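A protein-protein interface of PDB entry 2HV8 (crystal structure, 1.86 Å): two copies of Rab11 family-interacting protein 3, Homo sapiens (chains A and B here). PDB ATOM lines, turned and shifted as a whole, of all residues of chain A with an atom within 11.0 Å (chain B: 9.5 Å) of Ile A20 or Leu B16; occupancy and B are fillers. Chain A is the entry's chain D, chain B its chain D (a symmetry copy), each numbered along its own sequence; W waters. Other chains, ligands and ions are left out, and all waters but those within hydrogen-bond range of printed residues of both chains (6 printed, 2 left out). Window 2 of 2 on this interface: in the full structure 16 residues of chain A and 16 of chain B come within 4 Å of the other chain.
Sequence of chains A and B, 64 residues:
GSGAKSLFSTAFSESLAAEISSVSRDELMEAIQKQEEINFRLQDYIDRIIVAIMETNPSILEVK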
ATOM      1  N   PHE A  12      16.621  27.750  20.074  1.00  0.00           N
ATOM      2  CA  PHE A  12      17.099  27.089  18.863  1.00  0.00           C
ATOM      3  C   PHE A  12      15.984  26.689  17.882  1.00  0.00           C
ATOM      4  O   PHE A  12      16.075  26.981  16.686  1.00  0.00           O
ATOM      5  CB  PHE A  12      17.970  25.879  19.226  1.00  0.00           C
ATOM      6  CG  PHE A  12      18.360  25.038  18.048  1.00  0.00           C
ATOM      7  CD1 PHE A  12      19.337  25.475  17.160  1.00  0.00           C
ATOM      8  CD2 PHE A  12      17.748  23.812  17.825  1.00  0.00           C
ATOM      9  CE1 PHE A  12      19.694  24.701  16.070  1.00  0.00           C
ATOM     10  CE2 PHE A  12      18.098  23.034  16.734  1.00  0.00           C
ATOM     11  CZ  PHE A  12      19.071  23.478  15.857  1.00  0.00           C
ATOM     12  N   SER A  13      14.943  26.031  18.391  1.00  0.00           N
ATOM     13  CA  SER A  13      13.850  25.541  17.544  1.00  0.00           C
ATOM     14  C   SER A  13      13.100  26.674  16.843  1.00  0.00           C
ATOM     15  O   SER A  13      12.597  26.497  15.732  1.00  0.00           O
ATOM     16  CB  SER A  13      12.878  24.674  18.348  1.00  0.00           C
ATOM     17  OG  SER A  13      12.254  25.427  19.373  1.00  0.00           O
ATOM     18  N   GLU A  14      13.031  27.830  17.504  1.00  0.00           N
ATOM     19  CA  GLU A  14      12.434  29.040  16.933  1.00  0.00           C
ATOM     20  C   GLU A  14      13.323  29.647  15.846  1.00  0.00           C
ATOM     21  O   GLU A  14      12.832  30.079  14.798  1.00  0.00           O
ATOM     22  CB  GLU A  14      12.167  30.064  18.027  1.00  0.00           C
ATOM     23  N   SER A  15      14.628  29.681  16.109  1.00  0.00           N
ATOM     24  CA  SER A  15      15.609  30.204  15.156  1.00  0.00           C
ATOM     25  C   SER A  15      15.726  29.295  13.932  1.00  0.00           C
ATOM     26  O   SER A  15      15.929  29.770  12.811  1.00  0.00           O
ATOM     27  CB  SER A  15      16.966  30.388  15.834  1.00  0.00           C
ATOM     28  N   LEU A  16      15.587  27.988  14.154  1.00  0.00           N
ATOM     29  CA  LEU A  16      15.585  27.007  13.070  1.00  0.00           C
ATOM     30  C   LEU A  16      14.319  27.096  12.216  1.00  0.00           C
ATOM     31  O   LEU A  16      14.393  27.016  10.986  1.00  0.00           O
ATOM     32  CB  LEU A  16      15.740  25.584  13.624  1.00  0.00           C
ATOM     33  CG  LEU A  16      15.733  24.405  12.643  1.00  0.00           C
ATOM     34  CD1 LEU A  16      16.956  24.424  11.728  1.00  0.00           C
ATOM     35  CD2 LEU A  16      15.656  23.096  13.407  1.00  0.00           C
ATOM     36  N   ALA A  17      13.168  27.252  12.871  1.00  0.00           N
ATOM     37  CA  ALA A  17      11.872  27.319  12.183  1.00  0.00           C
ATOM     38  C   ALA A  17      11.814  28.448  11.155  1.00  0.00           C
ATOM     39  O   ALA A  17      11.280  28.268  10.054  1.00  0.00           O
ATOM     40  CB  ALA A  17      10.738  27.460  13.185  1.00  0.00           C
ATOM     41  N   ALA A  18      12.374  29.601  11.520  1.00  0.00           N
ATOM     42  CA  ALA A  18      12.394  30.783  10.658  1.00  0.00           C
ATOM     43  C   ALA A  18      13.224  30.572   9.392  1.00  0.00           C
ATOM     44  O   ALA A  18      13.071  31.306   8.414  1.00  0.00           O
ATOM     45  CB  ALA A  18      12.901  31.998  11.438  1.00  0.00           C
ATOM     46  N   GLU A  19      14.091  29.562   9.411  1.00  0.00           N
ATOM     47  CA  GLU A  19      14.959  29.267   8.274  1.00  0.00           C
ATOM     48  C   GLU A  19      14.447  28.130   7.389  1.00  0.00           C
ATOM     49  O   GLU A  19      15.080  27.777   6.394  1.00  0.00           O
ATOM     50  CB  GLU A  19      16.397  28.995   8.736  1.00  0.00           C
ATOM     51  CG  GLU A  19      17.051  30.148   9.504  1.00  0.00           C
ATOM     52  CD  GLU A  19      17.029  31.479   8.762  1.00  0.00           C
ATOM     53  OE1 GLU A  19      17.209  31.495   7.527  1.00  0.00           O
ATOM     54  OE2 GLU A  19      16.833  32.517   9.424  1.00  0.00           O
ATOM     55  N   ILE A  20      13.302  27.558   7.752  1.00  0.00           N
ATOM     56  CA  ILE A  20      12.716  26.474   6.967  1.00  0.00           C
ATOM     57  C   ILE A  20      11.487  26.953   6.197  1.00  0.00           C
ATOM     58  O   ILE A  20      10.466  27.318   6.788  1.00  0.00           O
ATOM     59  CB  ILE A  20      12.361  25.237   7.834  1.00  0.00           C
ATOM     60  CG1 ILE A  20      13.602  24.727   8.574  1.00  0.00           C
ATOM     61  CG2 ILE A  20      11.760  24.127   6.966  1.00  0.00           C
ATOM     62  CD1 ILE A  20      13.291  23.801   9.732  1.00  0.00           C
ATOM     63  N   SER A  21      11.608  26.952   4.874  1.00  0.00           N
ATOM     64  CA  SER A  21      10.503  27.304   3.993  1.00  0.00           C
ATOM     65  C   SER A  21       9.531  26.133   3.864  1.00  0.00           C
ATOM     66  O   SER A  21       9.926  24.972   3.993  1.00  0.00           O
ATOM     67  CB  SER A  21      11.029  27.709   2.625  1.00  0.00           C
ATOM     68  N   SER A  22       8.264  26.449   3.607  1.00  0.00           N
ATOM     69  CA  SER A  22       7.248  25.437   3.318  1.00  0.00           C
ATOM     70  C   SER A  22       7.546  24.733   1.994  1.00  0.00           C
ATOM     71  O   SER A  22       7.146  23.586   1.782  1.00  0.00           O
ATOM     72  CB  SER A  22       5.864  26.072   3.280  1.00  0.00           C
ATOM     73  N   VAL A  23       8.255  25.435   1.113  1.00  0.00           N
ATOM     74  CA  VAL A  23       8.638  24.906  -0.190  1.00  0.00           C
ATOM     75  C   VAL A  23      10.001  24.228  -0.087  1.00  0.00           C
ATOM     76  O   VAL A  23      10.892  24.720   0.608  1.00  0.00           O
ATOM     77  CB  VAL A  23       8.694  26.031  -1.260  1.00  0.00           C
ATOM     78  CG1 VAL A  23       8.742  25.445  -2.656  1.00  0.00           C
ATOM     79  CG2 VAL A  23       7.493  26.969  -1.129  1.00  0.00           C
ATOM     80  N   SER A  24      10.157  23.096  -0.773  1.00  0.00           N
ATOM     81  CA  SER A  24      11.443  22.404  -0.854  1.00  0.00           C
ATOM     82  C   SER A  24      12.501  23.283  -1.519  1.00  0.00           C
ATOM     83  O   SER A  24      12.201  24.028  -2.458  1.00  0.00           O
ATOM     84  CB  SER A  24      11.293  21.095  -1.610  1.00  0.00           C
ATOM     85  N   ARG A  25      13.736  23.190  -1.029  1.00  0.00           N
ATOM     86  CA  ARG A  25      14.850  23.981  -1.558  1.00  0.00           C
ATOM     87  C   ARG A  25      15.143  23.705  -3.032  1.00  0.00           C
ATOM     88  O   ARG A  25      15.637  24.585  -3.741  1.00  0.00           O
ATOM     89  CB  ARG A  25      16.117  23.775  -0.728  1.00  0.00           C
ATOM     90  CG  ARG A  25      16.191  24.637   0.527  1.00  0.00           C
ATOM     91  CD  ARG A  25      17.587  25.216   0.708  1.00  0.00           C
ATOM     92  NE  ARG A  25      18.631  24.201   0.594  1.00  0.00           N
ATOM     93  CZ  ARG A  25      19.887  24.446   0.233  1.00  0.00           C
ATOM     94  NH1 ARG A  25      20.276  25.681  -0.064  1.00  0.00           N
ATOM     95  NH2 ARG A  25      20.757  23.449   0.160  1.00  0.00           N
ATOM     96  N   ASP A  26      14.840  22.486  -3.477  1.00  0.00           N
ATOM     97  CA  ASP A  26      14.950  22.109  -4.887  1.00  0.00           C
ATOM     98  C   ASP A  26      13.987  22.925  -5.742  1.00  0.00           C
ATOM     99  O   ASP A  26      14.344  23.383  -6.829  1.00  0.00           O
ATOM    100  CB  ASP A  26      14.686  20.619  -5.062  1.00  0.00           C
ATOM    101  N   LEU A  28      12.619  25.828  -4.723  1.00  0.00           N
ATOM    102  CA  LEU A  28      13.056  27.214  -4.543  1.00  0.00           C
ATOM    103  C   LEU A  28      14.200  27.567  -5.492  1.00  0.00           C
ATOM    104  O   LEU A  28      14.247  28.675  -6.028  1.00  0.00           O
ATOM    105  CB  LEU A  28      13.473  27.473  -3.089  1.00  0.00           C
ATOM    106  CG  LEU A  28      12.393  27.443  -2.000  1.00  0.00           C
ATOM    107  CD1 LEU A  28      13.036  27.462  -0.618  1.00  0.00           C
ATOM    108  CD2 LEU A  28      11.400  28.594  -2.147  1.00  0.00           C
ATOM    109  N   ALA B  11      18.313   9.734   6.791  1.00  0.00           N
ATOM    110  CA  ALA B  11      18.008  10.109   8.206  1.00  0.00           C
ATOM    111  C   ALA B  11      17.541  11.559   8.310  1.00  0.00           C
ATOM    112  O   ALA B  11      17.703  12.345   7.369  1.00  0.00           O
ATOM    113  CB  ALA B  11      19.223   9.870   9.094  1.00  0.00           C
ATOM    114  N   PHE B  12      16.969  11.903   9.463  1.00  0.00           N
ATOM    115  CA  PHE B  12      16.376  13.217   9.694  1.00  0.00           C
ATOM    116  C   PHE B  12      17.354  14.389   9.517  1.00  0.00           C
ATOM    117  O   PHE B  12      17.041  15.360   8.821  1.00  0.00           O
ATOM    118  CB  PHE B  12      15.710  13.264  11.077  1.00  0.00           C
ATOM    119  CG  PHE B  12      15.228  14.626  11.471  1.00  0.00           C
ATOM    120  CD1 PHE B  12      14.079  15.163  10.900  1.00  0.00           C
ATOM    121  CD2 PHE B  12      15.924  15.375  12.411  1.00  0.00           C
ATOM    122  CE1 PHE B  12      13.637  16.423  11.261  1.00  0.00           C
ATOM    123  CE2 PHE B  12      15.489  16.638  12.775  1.00  0.00           C
ATOM    124  CZ  PHE B  12      14.345  17.162  12.200  1.00  0.00           C
ATOM    125  N   SER B  13      18.529  14.293  10.140  1.00  0.00           N
ATOM    126  CA  SER B  13      19.517  15.377  10.098  1.00  0.00           C
ATOM    127  C   SER B  13      20.018  15.656   8.680  1.00  0.00           C
ATOM    128  O   SER B  13      20.351  16.795   8.349  1.00  0.00           O
ATOM    129  CB  SER B  13      20.694  15.084  11.032  1.00  0.00           C
ATOM    130  OG  SER B  13      21.390  13.919  10.623  1.00  0.00           O
ATOM    131  N   GLU B  14      20.068  14.609   7.857  1.00  0.00           N
ATOM    132  CA  GLU B  14      20.432  14.723   6.443  1.00  0.00           C
ATOM    133  C   GLU B  14      19.319  15.385   5.627  1.00  0.00           C
ATOM    134  O   GLU B  14      19.585  16.227   4.764  1.00  0.00           O
ATOM    135  CB  GLU B  14      20.760  13.352   5.869  1.00  0.00           C
ATOM    136  N   SER B  15      18.078  14.991   5.904  1.00  0.00           N
ATOM    137  CA  SER B  15      16.905  15.553   5.231  1.00  0.00           C
ATOM    138  C   SER B  15      16.690  17.014   5.627  1.00  0.00           C
ATOM    139  O   SER B  15      16.260  17.832   4.809  1.00  0.00           O
ATOM    140  CB  SER B  15      15.663  14.715   5.533  1.00  0.00           C
ATOM    141  N   LEU B  16      17.004  17.336   6.882  1.00  0.00           N
ATOM    142  CA  LEU B  16      16.937  18.710   7.376  1.00  0.00           C
ATOM    143  C   LEU B  16      18.031  19.592   6.774  1.00  0.00           C
ATOM    144  O   LEU B  16      17.769  20.740   6.403  1.00  0.00           O
ATOM    145  CB  LEU B  16      17.027  18.741   8.909  1.00  0.00           C
ATOM    146  CG  LEU B  16      17.002  20.099   9.621  1.00  0.00           C
ATOM    147  CD1 LEU B  16      15.652  20.797   9.462  1.00  0.00           C
ATOM    148  CD2 LEU B  16      17.341  19.919  11.090  1.00  0.00           C
ATOM    149  N   ALA B  17      19.249  19.055   6.689  1.00  0.00           N
ATOM    150  CA  ALA B  17      20.402  19.798   6.163  1.00  0.00           C
ATOM    151  C   ALA B  17      20.172  20.305   4.740  1.00  0.00           C
ATOM    152  O   ALA B  17      20.538  21.439   4.410  1.00  0.00           O
ATOM    153  CB  ALA B  17      21.661  18.949   6.223  1.00  0.00           C
ATOM    154  N   ALA B  18      19.558  19.461   3.912  1.00  0.00           N
ATOM    155  CA  ALA B  18      19.272  19.786   2.514  1.00  0.00           C
ATOM    156  C   ALA B  18      18.277  20.938   2.371  1.00  0.00           C
ATOM    157  O   ALA B  18      18.190  21.562   1.312  1.00  0.00           O
ATOM    158  CB  ALA B  18      18.769  18.545   1.774  1.00  0.00           C
ATOM    159  N   GLU B  19      17.537  21.220   3.441  1.00  0.00           N
ATOM    160  CA  GLU B  19      16.535  22.281   3.429  1.00  0.00           C
ATOM    161  C   GLU B  19      17.016  23.589   4.059  1.00  0.00           C
ATOM    162  O   GLU B  19      16.273  24.569   4.114  1.00  0.00           O
ATOM    163  CB  GLU B  19      15.227  21.811   4.082  1.00  0.00           C
ATOM    164  CG  GLU B  19      14.586  20.588   3.417  1.00  0.00           C
ATOM    165  CD  GLU B  19      14.344  20.750   1.921  1.00  0.00           C
ATOM    166  OE1 GLU B  19      13.967  21.854   1.477  1.00  0.00           O
ATOM    167  OE2 GLU B  19      14.531  19.761   1.186  1.00  0.00           O
ATOM    168  N   ILE B  20      18.260  23.604   4.531  1.00  0.00           N
ATOM    169  CA  ILE B  20      18.825  24.808   5.137  1.00  0.00           C
ATOM    170  C   ILE B  20      19.854  25.457   4.216  1.00  0.00           C
ATOM    171  O   ILE B  20      20.912  24.884   3.936  1.00  0.00           O
ATOM    172  CB  ILE B  20      19.445  24.535   6.532  1.00  0.00           C
ATOM    173  CG1 ILE B  20      18.402  23.923   7.474  1.00  0.00           C
ATOM    174  CG2 ILE B  20      20.014  25.827   7.129  1.00  0.00           C
ATOM    175  CD1 ILE B  20      18.993  23.259   8.701  1.00  0.00           C
ATOM    176  N   SER B  21      19.523  26.654   3.744  1.00  0.00           N
ATOM    177  CA  SER B  21      20.427  27.441   2.918  1.00  0.00           C
ATOM    178  C   SER B  21      21.485  28.121   3.784  1.00  0.00           C
ATOM    179  O   SER B  21      21.244  28.413   4.958  1.00  0.00           O
ATOM    180  CB  SER B  21      19.646  28.478   2.125  1.00  0.00           C
ATOM    181  N   VAL B  23      22.369  31.046   3.197  1.00  0.00           N
ATOM    182  CA  VAL B  23      21.840  32.402   3.259  1.00  0.00           C
ATOM    183  C   VAL B  23      20.592  32.426   4.137  1.00  0.00           C
ATOM    184  O   VAL B  23      19.777  31.503   4.088  1.00  0.00           O
ATOM    185  CB  VAL B  23      21.491  32.936   1.842  1.00  0.00           C
ATOM    186  CG1 VAL B  23      21.282  34.436   1.867  1.00  0.00           C
ATOM    187  CG2 VAL B  23      22.590  32.580   0.838  1.00  0.00           C
ATOM    188  N   SER B  24      20.450  33.479   4.942  1.00  0.00           N
ATOM    189  CA  SER B  24      19.250  33.684   5.752  1.00  0.00           C
ATOM    190  C   SER B  24      18.010  33.836   4.872  1.00  0.00           C
ATOM    191  O   SER B  24      18.073  34.436   3.794  1.00  0.00           O
ATOM    192  CB  SER B  24      19.416  34.902   6.645  1.00  0.00           C
ATOM    193  N   ARG B  25      16.888  33.291   5.338  1.00  0.00           N
ATOM    194  CA  ARG B  25      15.624  33.347   4.598  1.00  0.00           C
ATOM    195  C   ARG B  25      15.129  34.770   4.351  1.00  0.00           C
ATOM    196  O   ARG B  25      14.435  35.023   3.363  1.00  0.00           O
ATOM    197  CB  ARG B  25      14.537  32.531   5.299  1.00  0.00           C
ATOM    198  CG  ARG B  25      14.574  31.040   4.988  1.00  0.00           C
ATOM    199  CD  ARG B  25      13.172  30.498   4.751  1.00  0.00           C
ATOM    200  NE  ARG B  25      12.239  30.886   5.805  1.00  0.00           N
ATOM    201  CZ  ARG B  25      10.921  30.985   5.649  1.00  0.00           C
ATOM    202  NH1 ARG B  25      10.360  30.734   4.473  1.00  0.00           N
ATOM    203  NH2 ARG B  25      10.164  31.348   6.675  1.00  0.00           N
ATOM    204  N   ASP B  26      15.486  35.685   5.251  1.00  0.00           N
ATOM    205  CA  ASP B  26      15.191  37.110   5.091  1.00  0.00           C
ATOM    206  C   ASP B  26      15.910  37.678   3.872  1.00  0.00           C
ATOM    207  O   ASP B  26      15.335  38.455   3.108  1.00  0.00           O
ATOM    208  CB  ASP B  26      15.582  37.880   6.346  1.00  0.00           C
ATOM    209  N   LEU B  28      17.104  35.760   1.375  1.00  0.00           N
ATOM    210  CA  LEU B  28      16.556  35.009   0.245  1.00  0.00           C
ATOM    211  C   LEU B  28      15.243  35.616  -0.246  1.00  0.00           C
ATOM    212  O   LEU B  28      14.991  35.669  -1.450  1.00  0.00           O
ATOM    213  CB  LEU B  28      16.353  33.533   0.615  1.00  0.00           C
ATOM    214  CG  LEU B  28      17.592  32.665   0.872  1.00  0.00           C
ATOM    215  CD1 LEU B  28      17.181  31.324   1.471  1.00  0.00           C
ATOM    216  CD2 LEU B  28      18.418  32.457  -0.395  1.00  0.00           C
HETATM  217  O   HOH W   1       9.291  29.500   8.550  1.00  0.00           O
HETATM  218  O   HOH W   2      15.947  34.762   8.238  1.00  0.00           O
HETATM  219  O   HOH W   3      14.089  25.994   3.462  1.00  0.00           O
HETATM  220  O   HOH W   4      16.964  28.052   4.497  1.00  0.00           O
HETATM  221  O   HOH W   5      14.969  20.065  -1.450  1.00  0.00           O
HETATM  222  O   HOH W   6      22.114  22.548   2.405  1.00  0.00           O
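Water W4 lies within hydrogen-bond range of the backbone carbonyl oxygen (O) of Glu A19 (2.7 Å) and the backbone NH (N) of Ser B21 (3.0 Å).
Water W3 lies within hydrogen-bond range of O of Glu B19 (2.7 Å) and N of Ser A21 (3.0 Å).
Water W2 lies within hydrogen-bond range of OE2 of Glu A19, N of Asp B26 and N of Arg B25.
Water W5 lies within hydrogen-bond range of OE2 of Glu B19 (2.7 Å), N of Asp A26 (3.2 Å) and N of Arg A25 (3.4 Å).
Water W6 lies within hydrogen-bond range of the guanidinium group (NH2) of Arg A25 (2.8 Å), the backbone carbonyl oxygen (O) of Ala B17 (2.8 Å) and the backbone carbonyl oxygen (O) of Ile B20 (3.0 Å).
Water W1 lies within hydrogen-bond range of the guanidinium group of Arg B25 (2.8 Å), the backbone carbonyl oxygen of Ala A17 (2.8 Å) and the backbone carbonyl oxygen of Ile A20 (3.0 Å).
Ala A18 touches Arg B25, and with the chains exchanged Arg A25 touches Ala B18.
Glu A19 touches Ser B24, and with the chains exchanged Ser A24 touches Glu B19.
Ile A20 touches Arg B25, and with the chains exchanged Arg A25 touches Ile B20.
Ser A21 touches Arg B25, and with the chains exchanged Arg A25 touches Ser B21.
Positions printed for both chains: 12, 13, 14, 15, 16, 17, 18, 19, 20, 21, 23, 24, 25, 26 and 28.
The side-chain carboxylate (OE1) of Glu B19 sits at hydrogen-bond distance from the backbone NH (N) of Arg A25 (2.8 Å).
The guanidinium group (NE) of Arg A25 is in hydrogen-bond range of the backbone carbonyl oxygen (O) of Ala B18 (2.8 Å).
NE of Arg B25 is in hydrogen-bond range of O of Ala A18 (2.8 Å).
OE1 of Glu A19 sits at hydrogen-bond distance from N of Arg B25 (2.8 Å).
Ile A20 touches two residues of chain B.
Of chain B, only Arg B25 (3.5 Å) comes within 4 Å of Ser A21.
Val A23 touches none of the printed residues of chain B.
Printed residues of chain B within 4 Å of Ser A24: Glu B19.
Of the printed residues of chain B, Arg A25 touches Ala B18, Glu B19, Ile B20 and Ser B21.
No residue of chain A comes within 4 Å of Phe B12.
Leu B16 touches just one residue of chain A: Ile A20.
No residue of chain A comes within 4 Å of Ala B17.
Of chain A, only Arg A25 comes within 4 Å of Ala B18.
Of chain A, only Ser A24 (3.5 Å) and Arg A25 (2.8 Å) come within 4 Å of Glu B19.
Of the printed residues of chain A, Ser B24 touches Glu A19 (3.5 Å).
The nearest printed residue of chain A that does not touch Ser B21 is Glu A19 (5.3 Å).
Of the 16 printed residues of chain B, 7 touch a printed residue of chain A.
Hydrophobic or aromatic side chains of chain B that line the printed part of chain A: Leu B16 and Ile B20.
Hydrophobic or aromatic side chains of chain A that line the printed part of chain B: Leu A16 and Ile A20.
Among the printed residues, no Asp or Glu carboxylate lies within 4 Å of a Lys or Arg side-chain nitrogen of the other chain.
Ile B20 touches Leu A16 (CD1 to CD1, 3.8 Å).
Glu A19 touches Ser B24.
Leu B16 touches Ile A20 (CD1 to CD1, 3.8 Å).
Arg B25 touches Ile A20 (CZ to O, 3.9 Å).
Ser A21 touches Arg B25 (CA to NH1, 3.5 Å).
Ser A24 touches Glu B19.
Arg A25 touches Ile B20.
Arg A25 touches Ser B21 (NH1 to CA, 3.5 Å).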
